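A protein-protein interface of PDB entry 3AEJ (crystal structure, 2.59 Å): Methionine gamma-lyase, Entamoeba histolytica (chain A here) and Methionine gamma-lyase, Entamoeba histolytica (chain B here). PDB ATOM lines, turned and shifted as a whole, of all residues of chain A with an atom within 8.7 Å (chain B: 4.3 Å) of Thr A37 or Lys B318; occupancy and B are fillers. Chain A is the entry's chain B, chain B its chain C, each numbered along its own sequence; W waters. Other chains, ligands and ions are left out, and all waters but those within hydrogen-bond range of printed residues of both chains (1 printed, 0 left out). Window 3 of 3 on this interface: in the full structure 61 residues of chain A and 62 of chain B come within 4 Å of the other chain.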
ATOM      1  N   PHE A  34       8.196 -12.358   0.788  1.00  0.00           N
ATOM      2  CA  PHE A  34       9.388 -11.570   0.493  1.00  0.00           C
ATOM      3  C   PHE A  34       9.377 -10.248   1.259  1.00  0.00           C
ATOM      4  O   PHE A  34       8.316  -9.665   1.485  1.00  0.00           O
ATOM      5  CB  PHE A  34       9.505 -11.300  -1.011  1.00  0.00           C
ATOM      6  CG  PHE A  34       9.738 -12.534  -1.843  1.00  0.00           C
ATOM      7  CD1 PHE A  34      10.637 -13.516  -1.433  1.00  0.00           C
ATOM      8  CD2 PHE A  34       9.079 -12.697  -3.059  1.00  0.00           C
ATOM      9  CE1 PHE A  34      10.860 -14.655  -2.211  1.00  0.00           C
ATOM     10  CE2 PHE A  34       9.297 -13.829  -3.846  1.00  0.00           C
ATOM     11  CZ  PHE A  34      10.189 -14.810  -3.419  1.00  0.00           C
ATOM     12  N   ASP A  35      10.562  -9.788   1.656  1.00  0.00           N
ATOM     13  CA  ASP A  35      10.714  -8.502   2.341  1.00  0.00           C
ATOM     14  C   ASP A  35      10.589  -7.347   1.356  1.00  0.00           C
ATOM     15  O   ASP A  35      10.082  -6.278   1.698  1.00  0.00           O
ATOM     16  CB  ASP A  35      12.071  -8.424   3.051  1.00  0.00           C
ATOM     17  CG  ASP A  35      12.253  -9.508   4.101  1.00  0.00           C
ATOM     18  OD1 ASP A  35      11.305  -9.771   4.873  1.00  0.00           O
ATOM     19  OD2 ASP A  35      13.355 -10.092   4.162  1.00  0.00           O
ATOM     20  N   SER A  36      11.065  -7.579   0.134  1.00  0.00           N
ATOM     21  CA  SER A  36      11.068  -6.580  -0.930  1.00  0.00           C
ATOM     22  C   SER A  36      11.142  -7.260  -2.297  1.00  0.00           C
ATOM     23  O   SER A  36      11.334  -8.477  -2.384  1.00  0.00           O
ATOM     24  CB  SER A  36      12.250  -5.619  -0.759  1.00  0.00           C
ATOM     25  OG  SER A  36      13.487  -6.311  -0.800  1.00  0.00           O
ATOM     26  N   THR A  37      10.981  -6.469  -3.356  1.00  0.00           N
ATOM     27  CA  THR A  37      11.126  -6.955  -4.725  1.00  0.00           C
ATOM     28  C   THR A  37      12.538  -7.493  -4.955  1.00  0.00           C
ATOM     29  O   THR A  37      12.711  -8.598  -5.474  1.00  0.00           O
ATOM     30  CB  THR A  37      10.836  -5.843  -5.757  1.00  0.00           C
ATOM     31  OG1 THR A  37       9.623  -5.166  -5.409  1.00  0.00           O
ATOM     32  CG2 THR A  37      10.711  -6.424  -7.163  1.00  0.00           C
ATOM     33  N   GLN A  38      13.535  -6.704  -4.550  1.00  0.00           N
ATOM     34  CA  GLN A  38      14.944  -7.049  -4.733  1.00  0.00           C
ATOM     35  C   GLN A  38      15.320  -8.328  -3.989  1.00  0.00           C
ATOM     36  O   GLN A  38      16.076  -9.149  -4.508  1.00  0.00           O
ATOM     37  CB  GLN A  38      15.846  -5.881  -4.300  1.00  0.00           C
ATOM     38  CG  GLN A  38      17.335  -6.066  -4.603  1.00  0.00           C
ATOM     39  CD  GLN A  38      17.629  -6.228  -6.088  1.00  0.00           C
ATOM     40  OE1 GLN A  38      17.240  -5.396  -6.908  1.00  0.00           O
ATOM     41  NE2 GLN A  38      18.326  -7.303  -6.437  1.00  0.00           N
ATOM     42  N   GLN A  39      14.780  -8.493  -2.782  1.00  0.00           N
ATOM     43  CA  GLN A  39      15.039  -9.674  -1.959  1.00  0.00           C
ATOM     44  C   GLN A  39      14.466 -10.935  -2.608  1.00  0.00           C
ATOM     45  O   GLN A  39      15.098 -11.994  -2.587  1.00  0.00           O
ATOM     46  CB  GLN A  39      14.477  -9.470  -0.549  1.00  0.00           C
ATOM     47  CG  GLN A  39      14.948 -10.483   0.490  1.00  0.00           C
ATOM     48  CD  GLN A  39      13.961 -11.615   0.710  1.00  0.00           C
ATOM     49  OE1 GLN A  39      12.774 -11.497   0.397  1.00  0.00           O
ATOM     50  NE2 GLN A  39      14.447 -12.721   1.262  1.00  0.00           N
ATOM     51  N   GLY A  40      13.274 -10.803  -3.188  1.00  0.00           N
ATOM     52  CA  GLY A  40      12.623 -11.891  -3.913  1.00  0.00           C
ATOM     53  C   GLY A  40      13.319 -12.216  -5.218  1.00  0.00           C
ATOM     54  O   GLY A  40      13.559 -13.386  -5.526  1.00  0.00           O
ATOM     55  N   ALA A  41      13.647 -11.175  -5.984  1.00  0.00           N
ATOM     56  CA  ALA A  41      14.379 -11.321  -7.243  1.00  0.00           C
ATOM     57  C   ALA A  41      15.759 -11.931  -7.023  1.00  0.00           C
ATOM     58  O   ALA A  41      16.245 -12.698  -7.860  1.00  0.00           O
ATOM     59  CB  ALA A  41      14.498  -9.978  -7.950  1.00  0.00           C
ATOM     60  N   ASP A  42      16.381 -11.582  -5.897  1.00  0.00           N
ATOM     61  CA  ASP A  42      17.686 -12.122  -5.517  1.00  0.00           C
ATOM     62  C   ASP A  42      17.635 -13.628  -5.271  1.00  0.00           C
ATOM     63  O   ASP A  42      18.486 -14.357  -5.768  1.00  0.00           O
ATOM     64  CB  ASP A  42      18.238 -11.403  -4.280  1.00  0.00           C
ATOM     65  CG  ASP A  42      18.975 -10.117  -4.619  1.00  0.00           C
ATOM     66  OD1 ASP A  42      19.143  -9.806  -5.819  1.00  0.00           O
ATOM     67  OD2 ASP A  42      19.393  -9.415  -3.674  1.00  0.00           O
ATOM     68  N   LEU A  43      16.631 -14.080  -4.518  1.00  0.00           N
ATOM     69  CA  LEU A  43      16.487 -15.497  -4.158  1.00  0.00           C
ATOM     70  C   LEU A  43      16.313 -16.429  -5.358  1.00  0.00           C
ATOM     71  O   LEU A  43      16.679 -17.604  -5.293  1.00  0.00           O
ATOM     72  CB  LEU A  43      15.335 -15.694  -3.165  1.00  0.00           C
ATOM     73  CG  LEU A  43      15.593 -15.365  -1.690  1.00  0.00           C
ATOM     74  CD1 LEU A  43      14.294 -15.410  -0.903  1.00  0.00           C
ATOM     75  CD2 LEU A  43      16.621 -16.307  -1.072  1.00  0.00           C
ATOM     76  N   PHE A  44      15.763 -15.899  -6.447  1.00  0.00           N
ATOM     77  CA  PHE A  44      15.580 -16.661  -7.679  1.00  0.00           C
ATOM     78  C   PHE A  44      16.869 -16.852  -8.491  1.00  0.00           C
ATOM     79  O   PHE A  44      16.848 -17.501  -9.539  1.00  0.00           O
ATOM     80  CB  PHE A  44      14.517 -15.993  -8.557  1.00  0.00           C
ATOM     81  CG  PHE A  44      13.123 -16.500  -8.322  1.00  0.00           C
ATOM     82  CD1 PHE A  44      12.233 -15.785  -7.527  1.00  0.00           C
ATOM     83  CD2 PHE A  44      12.693 -17.687  -8.908  1.00  0.00           C
ATOM     84  CE1 PHE A  44      10.939 -16.247  -7.315  1.00  0.00           C
ATOM     85  CE2 PHE A  44      11.402 -18.159  -8.699  1.00  0.00           C
ATOM     86  CZ  PHE A  44      10.523 -17.436  -7.905  1.00  0.00           C
ATOM     87  N   PHE B 314       8.920   0.328 -13.880  1.00  0.00           N
ATOM     88  CA  PHE B 314       9.392  -0.665 -12.923  1.00  0.00           C
ATOM     89  C   PHE B 314       9.379  -0.111 -11.497  1.00  0.00           C
ATOM     90  O   PHE B 314       8.948  -0.790 -10.565  1.00  0.00           O
ATOM     91  CB  PHE B 314      10.794  -1.154 -13.305  1.00  0.00           C
ATOM     92  CG  PHE B 314      11.510  -1.886 -12.200  1.00  0.00           C
ATOM     93  CD1 PHE B 314      12.628  -1.322 -11.590  1.00  0.00           C
ATOM     94  CD2 PHE B 314      11.065  -3.131 -11.766  1.00  0.00           C
ATOM     95  CE1 PHE B 314      13.293  -1.987 -10.566  1.00  0.00           C
ATOM     96  CE2 PHE B 314      11.722  -3.805 -10.739  1.00  0.00           C
ATOM     97  CZ  PHE B 314      12.838  -3.233 -10.139  1.00  0.00           C
ATOM     98  N   GLU B 315       9.845   1.127 -11.343  1.00  0.00           N
ATOM     99  CA  GLU B 315       9.924   1.780 -10.035  1.00  0.00           C
ATOM    100  C   GLU B 315       8.545   1.990  -9.409  1.00  0.00           C
ATOM    101  O   GLU B 315       8.390   1.876  -8.193  1.00  0.00           O
ATOM    102  CB  GLU B 315      10.680   3.110 -10.139  1.00  0.00           C
ATOM    103  CG  GLU B 315      12.198   2.974 -10.319  1.00  0.00           C
ATOM    104  CD  GLU B 315      12.616   2.494 -11.710  1.00  0.00           C
ATOM    105  OE1 GLU B 315      11.807   2.583 -12.660  1.00  0.00           O
ATOM    106  OE2 GLU B 315      13.768   2.030 -11.853  1.00  0.00           O
ATOM    107  N   ALA B 316       7.554   2.290 -10.248  1.00  0.00           N
ATOM    108  CA  ALA B 316       6.171   2.444  -9.800  1.00  0.00           C
ATOM    109  C   ALA B 316       5.584   1.100  -9.365  1.00  0.00           C
ATOM    110  O   ALA B 316       4.858   1.022  -8.372  1.00  0.00           O
ATOM    111  CB  ALA B 316       5.322   3.073 -10.895  1.00  0.00           C
ATOM    112  N   ALA B 317       5.910   0.052 -10.117  1.00  0.00           N
ATOM    113  CA  ALA B 317       5.503  -1.312  -9.798  1.00  0.00           C
ATOM    114  C   ALA B 317       6.137  -1.767  -8.487  1.00  0.00           C
ATOM    115  O   ALA B 317       5.490  -2.419  -7.667  1.00  0.00           O
ATOM    116  CB  ALA B 317       5.890  -2.251 -10.932  1.00  0.00           C
ATOM    117  N   LYS B 318       7.408  -1.411  -8.311  1.00  0.00           N
ATOM    118  CA  LYS B 318       8.172  -1.682  -7.094  1.00  0.00           C
ATOM    119  C   LYS B 318       7.586  -0.920  -5.906  1.00  0.00           C
ATOM    120  O   LYS B 318       7.593  -1.416  -4.780  1.00  0.00           O
ATOM    121  CB  LYS B 318       9.638  -1.290  -7.323  1.00  0.00           C
ATOM    122  CG  LYS B 318      10.567  -1.407  -6.126  1.00  0.00           C
ATOM    123  CD  LYS B 318      11.943  -0.844  -6.475  1.00  0.00           C
ATOM    124  CE  LYS B 318      12.899  -0.865  -5.287  1.00  0.00           C
ATOM    125  NZ  LYS B 318      12.515   0.101  -4.219  1.00  0.00           N
ATOM    126  N   LYS B 319       7.071   0.280  -6.171  1.00  0.00           N
ATOM    127  CA  LYS B 319       6.461   1.116  -5.140  1.00  0.00           C
ATOM    128  C   LYS B 319       5.136   0.532  -4.653  1.00  0.00           C
ATOM    129  O   LYS B 319       4.860   0.524  -3.454  1.00  0.00           O
ATOM    130  CB  LYS B 319       6.256   2.540  -5.656  1.00  0.00           C
ATOM    131  CG  LYS B 319       6.060   3.575  -4.562  1.00  0.00           C
ATOM    132  CD  LYS B 319       6.129   4.979  -5.122  1.00  0.00           C
ATOM    133  CE  LYS B 319       6.082   6.007  -4.011  1.00  0.00           C
ATOM    134  NZ  LYS B 319       6.205   7.383  -4.549  1.00  0.00           N
ATOM    135  N   LEU B 320       4.323   0.043  -5.588  1.00  0.00           N
ATOM    136  CA  LEU B 320       3.039  -0.562  -5.253  1.00  0.00           C
ATOM    137  C   LEU B 320       3.221  -1.835  -4.423  1.00  0.00           C
ATOM    138  O   LEU B 320       2.684  -1.950  -3.318  1.00  0.00           O
ATOM    139  CB  LEU B 320       2.234  -0.858  -6.524  1.00  0.00           C
ATOM    140  CG  LEU B 320       0.929  -1.649  -6.371  1.00  0.00           C
ATOM    141  CD1 LEU B 320      -0.142  -0.813  -5.684  1.00  0.00           C
ATOM    142  CD2 LEU B 320       0.439  -2.142  -7.718  1.00  0.00           C
ATOM    143  N   MET B 321       4.001  -2.768  -4.964  1.00  0.00           N
ATOM    144  CA  MET B 321       4.219  -4.085  -4.368  1.00  0.00           C
ATOM    145  C   MET B 321       4.770  -4.076  -2.941  1.00  0.00           C
ATOM    146  O   MET B 321       4.447  -4.960  -2.148  1.00  0.00           O
ATOM    147  CB  MET B 321       5.144  -4.906  -5.268  1.00  0.00           C
ATOM    148  CG  MET B 321       4.429  -5.691  -6.352  1.00  0.00           C
ATOM    149  SD  MET B 321       5.484  -6.144  -7.744  1.00  0.00           S
ATOM    150  CE  MET B 321       7.000  -6.614  -6.917  1.00  0.00           C
ATOM    151  N   GLU B 322       5.594  -3.081  -2.623  1.00  0.00           N
ATOM    152  CA  GLU B 322       6.328  -3.040  -1.353  1.00  0.00           C
ATOM    153  C   GLU B 322       5.652  -2.236  -0.248  1.00  0.00           C
ATOM    154  O   GLU B 322       6.158  -2.177   0.873  1.00  0.00           O
ATOM    155  CB  GLU B 322       7.740  -2.497  -1.577  1.00  0.00           C
ATOM    156  CG  GLU B 322       8.639  -3.433  -2.353  1.00  0.00           C
ATOM    157  CD  GLU B 322       9.999  -2.845  -2.632  1.00  0.00           C
ATOM    158  OE1 GLU B 322      10.778  -3.499  -3.351  1.00  0.00           O
ATOM    159  OE2 GLU B 322      10.296  -1.736  -2.138  1.00  0.00           O
ATOM    160  N   LEU B 329       3.422  -9.830  -0.527  1.00  0.00           N
ATOM    161  CA  LEU B 329       4.397 -10.024  -1.600  1.00  0.00           C
ATOM    162  C   LEU B 329       5.003 -11.426  -1.561  1.00  0.00           C
ATOM    163  O   LEU B 329       5.782 -11.753  -0.660  1.00  0.00           O
ATOM    164  CB  LEU B 329       5.490  -8.953  -1.513  1.00  0.00           C
ATOM    165  CG  LEU B 329       6.597  -8.899  -2.570  1.00  0.00           C
ATOM    166  CD1 LEU B 329       6.037  -8.614  -3.959  1.00  0.00           C
ATOM    167  CD2 LEU B 329       7.615  -7.844  -2.179  1.00  0.00           C
ATOM    168  N   MET B 346      10.696 -12.748 -10.932  1.00  0.00           N
ATOM    169  CA  MET B 346      10.359 -13.838 -10.013  1.00  0.00           C
ATOM    170  C   MET B 346       9.908 -15.117 -10.731  1.00  0.00           C
ATOM    171  O   MET B 346      10.731 -15.995 -10.997  1.00  0.00           O
ATOM    172  CB  MET B 346       9.336 -13.380  -8.961  1.00  0.00           C
ATOM    173  CG  MET B 346       9.855 -12.309  -8.001  1.00  0.00           C
ATOM    174  SD  MET B 346       8.554 -11.459  -7.081  1.00  0.00           S
ATOM    175  CE  MET B 346       9.509 -10.210  -6.222  1.00  0.00           C
HETATM  176  O   HOH W   1      13.140  -3.947  -4.071  1.00  0.00           O
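The backbone NH (N) of Phe A34 sits at hydrogen-bond distance from the backbone carbonyl oxygen (O) of Leu B329 (2.9 Å).
OG1 of Thr A37 sits at hydrogen-bond distance from OE1 of Glu B322 (2.9 Å).
OG of Ser A36 lies within hydrogen-bond range of N of Gln A39, 3.2 Å away.
The side-chain carboxylate (OE2) of Glu B322 lies within salt-bridge range of the side-chain amino group (NZ) of Lys B318.
Among the printed residues, merely in contact across the chains: Phe A44 with Met B346 (3.2 Å), Thr A37 with Met B321 (3.4 Å), Ser A36 with Leu B329 (3.6 Å), Ser A36 with Glu B322 (3.7 Å), Thr A37 with Met B346 (3.7 Å), Thr A37 with Leu B329 (3.8 Å) and Thr A37 with Lys B318 (3.9 Å).
Thr A37 touches just these residues of chain B: Lys B318, Met B321, Glu B322, Leu B329 and Met B346.
Lys B318 touches just one residue of chain A: Thr A37 (3.9 Å).
Ala B317 touches none of the printed residues of chain A.
Printed residues of chain A within 4 Å of Met B346: Thr A37 and Phe A44.
Of the printed residues of chain B, Phe A44 touches Met B346 (3.2 Å).
Of the printed residues of chain B, Ser A36 touches Glu B322 (3.7 Å) and Leu B329 (3.6 Å).
Of the printed residues of chain B, Phe A34 touches Leu B329.
The nearest printed residue of chain B that does not touch Thr A37 is Phe B314 (4.5 Å).
The nearest residue of chain A that does not touch Lys B318 is Gln A38 (5.9 Å).
The nearest printed residue of chain A that does not touch Met B346 is Phe A34 (4.05 Å).
Of the 11 printed residues of chain B, 5 touch a printed residue of chain A.
Hydrophobic or aromatic side chains of chain B within 4 Å of the printed part of chain A: Met B321, Leu B329 and Met B346.
Along chain B the printed residues that touch a printed residue of chain A span positions 318 to 346.
Of the 11 printed residues of chain A, 4 touch a printed residue of chain B.
Along chain A the printed residues that touch a printed residue of chain B span positions 34 to 44.
Water W1 lies within hydrogen-bond range of the side-chain carboxylate of Glu B322 (2.5 Å), the backbone NH of Gln A38 (2.8 Å) and the backbone NH of Thr A37 (3.4 Å).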
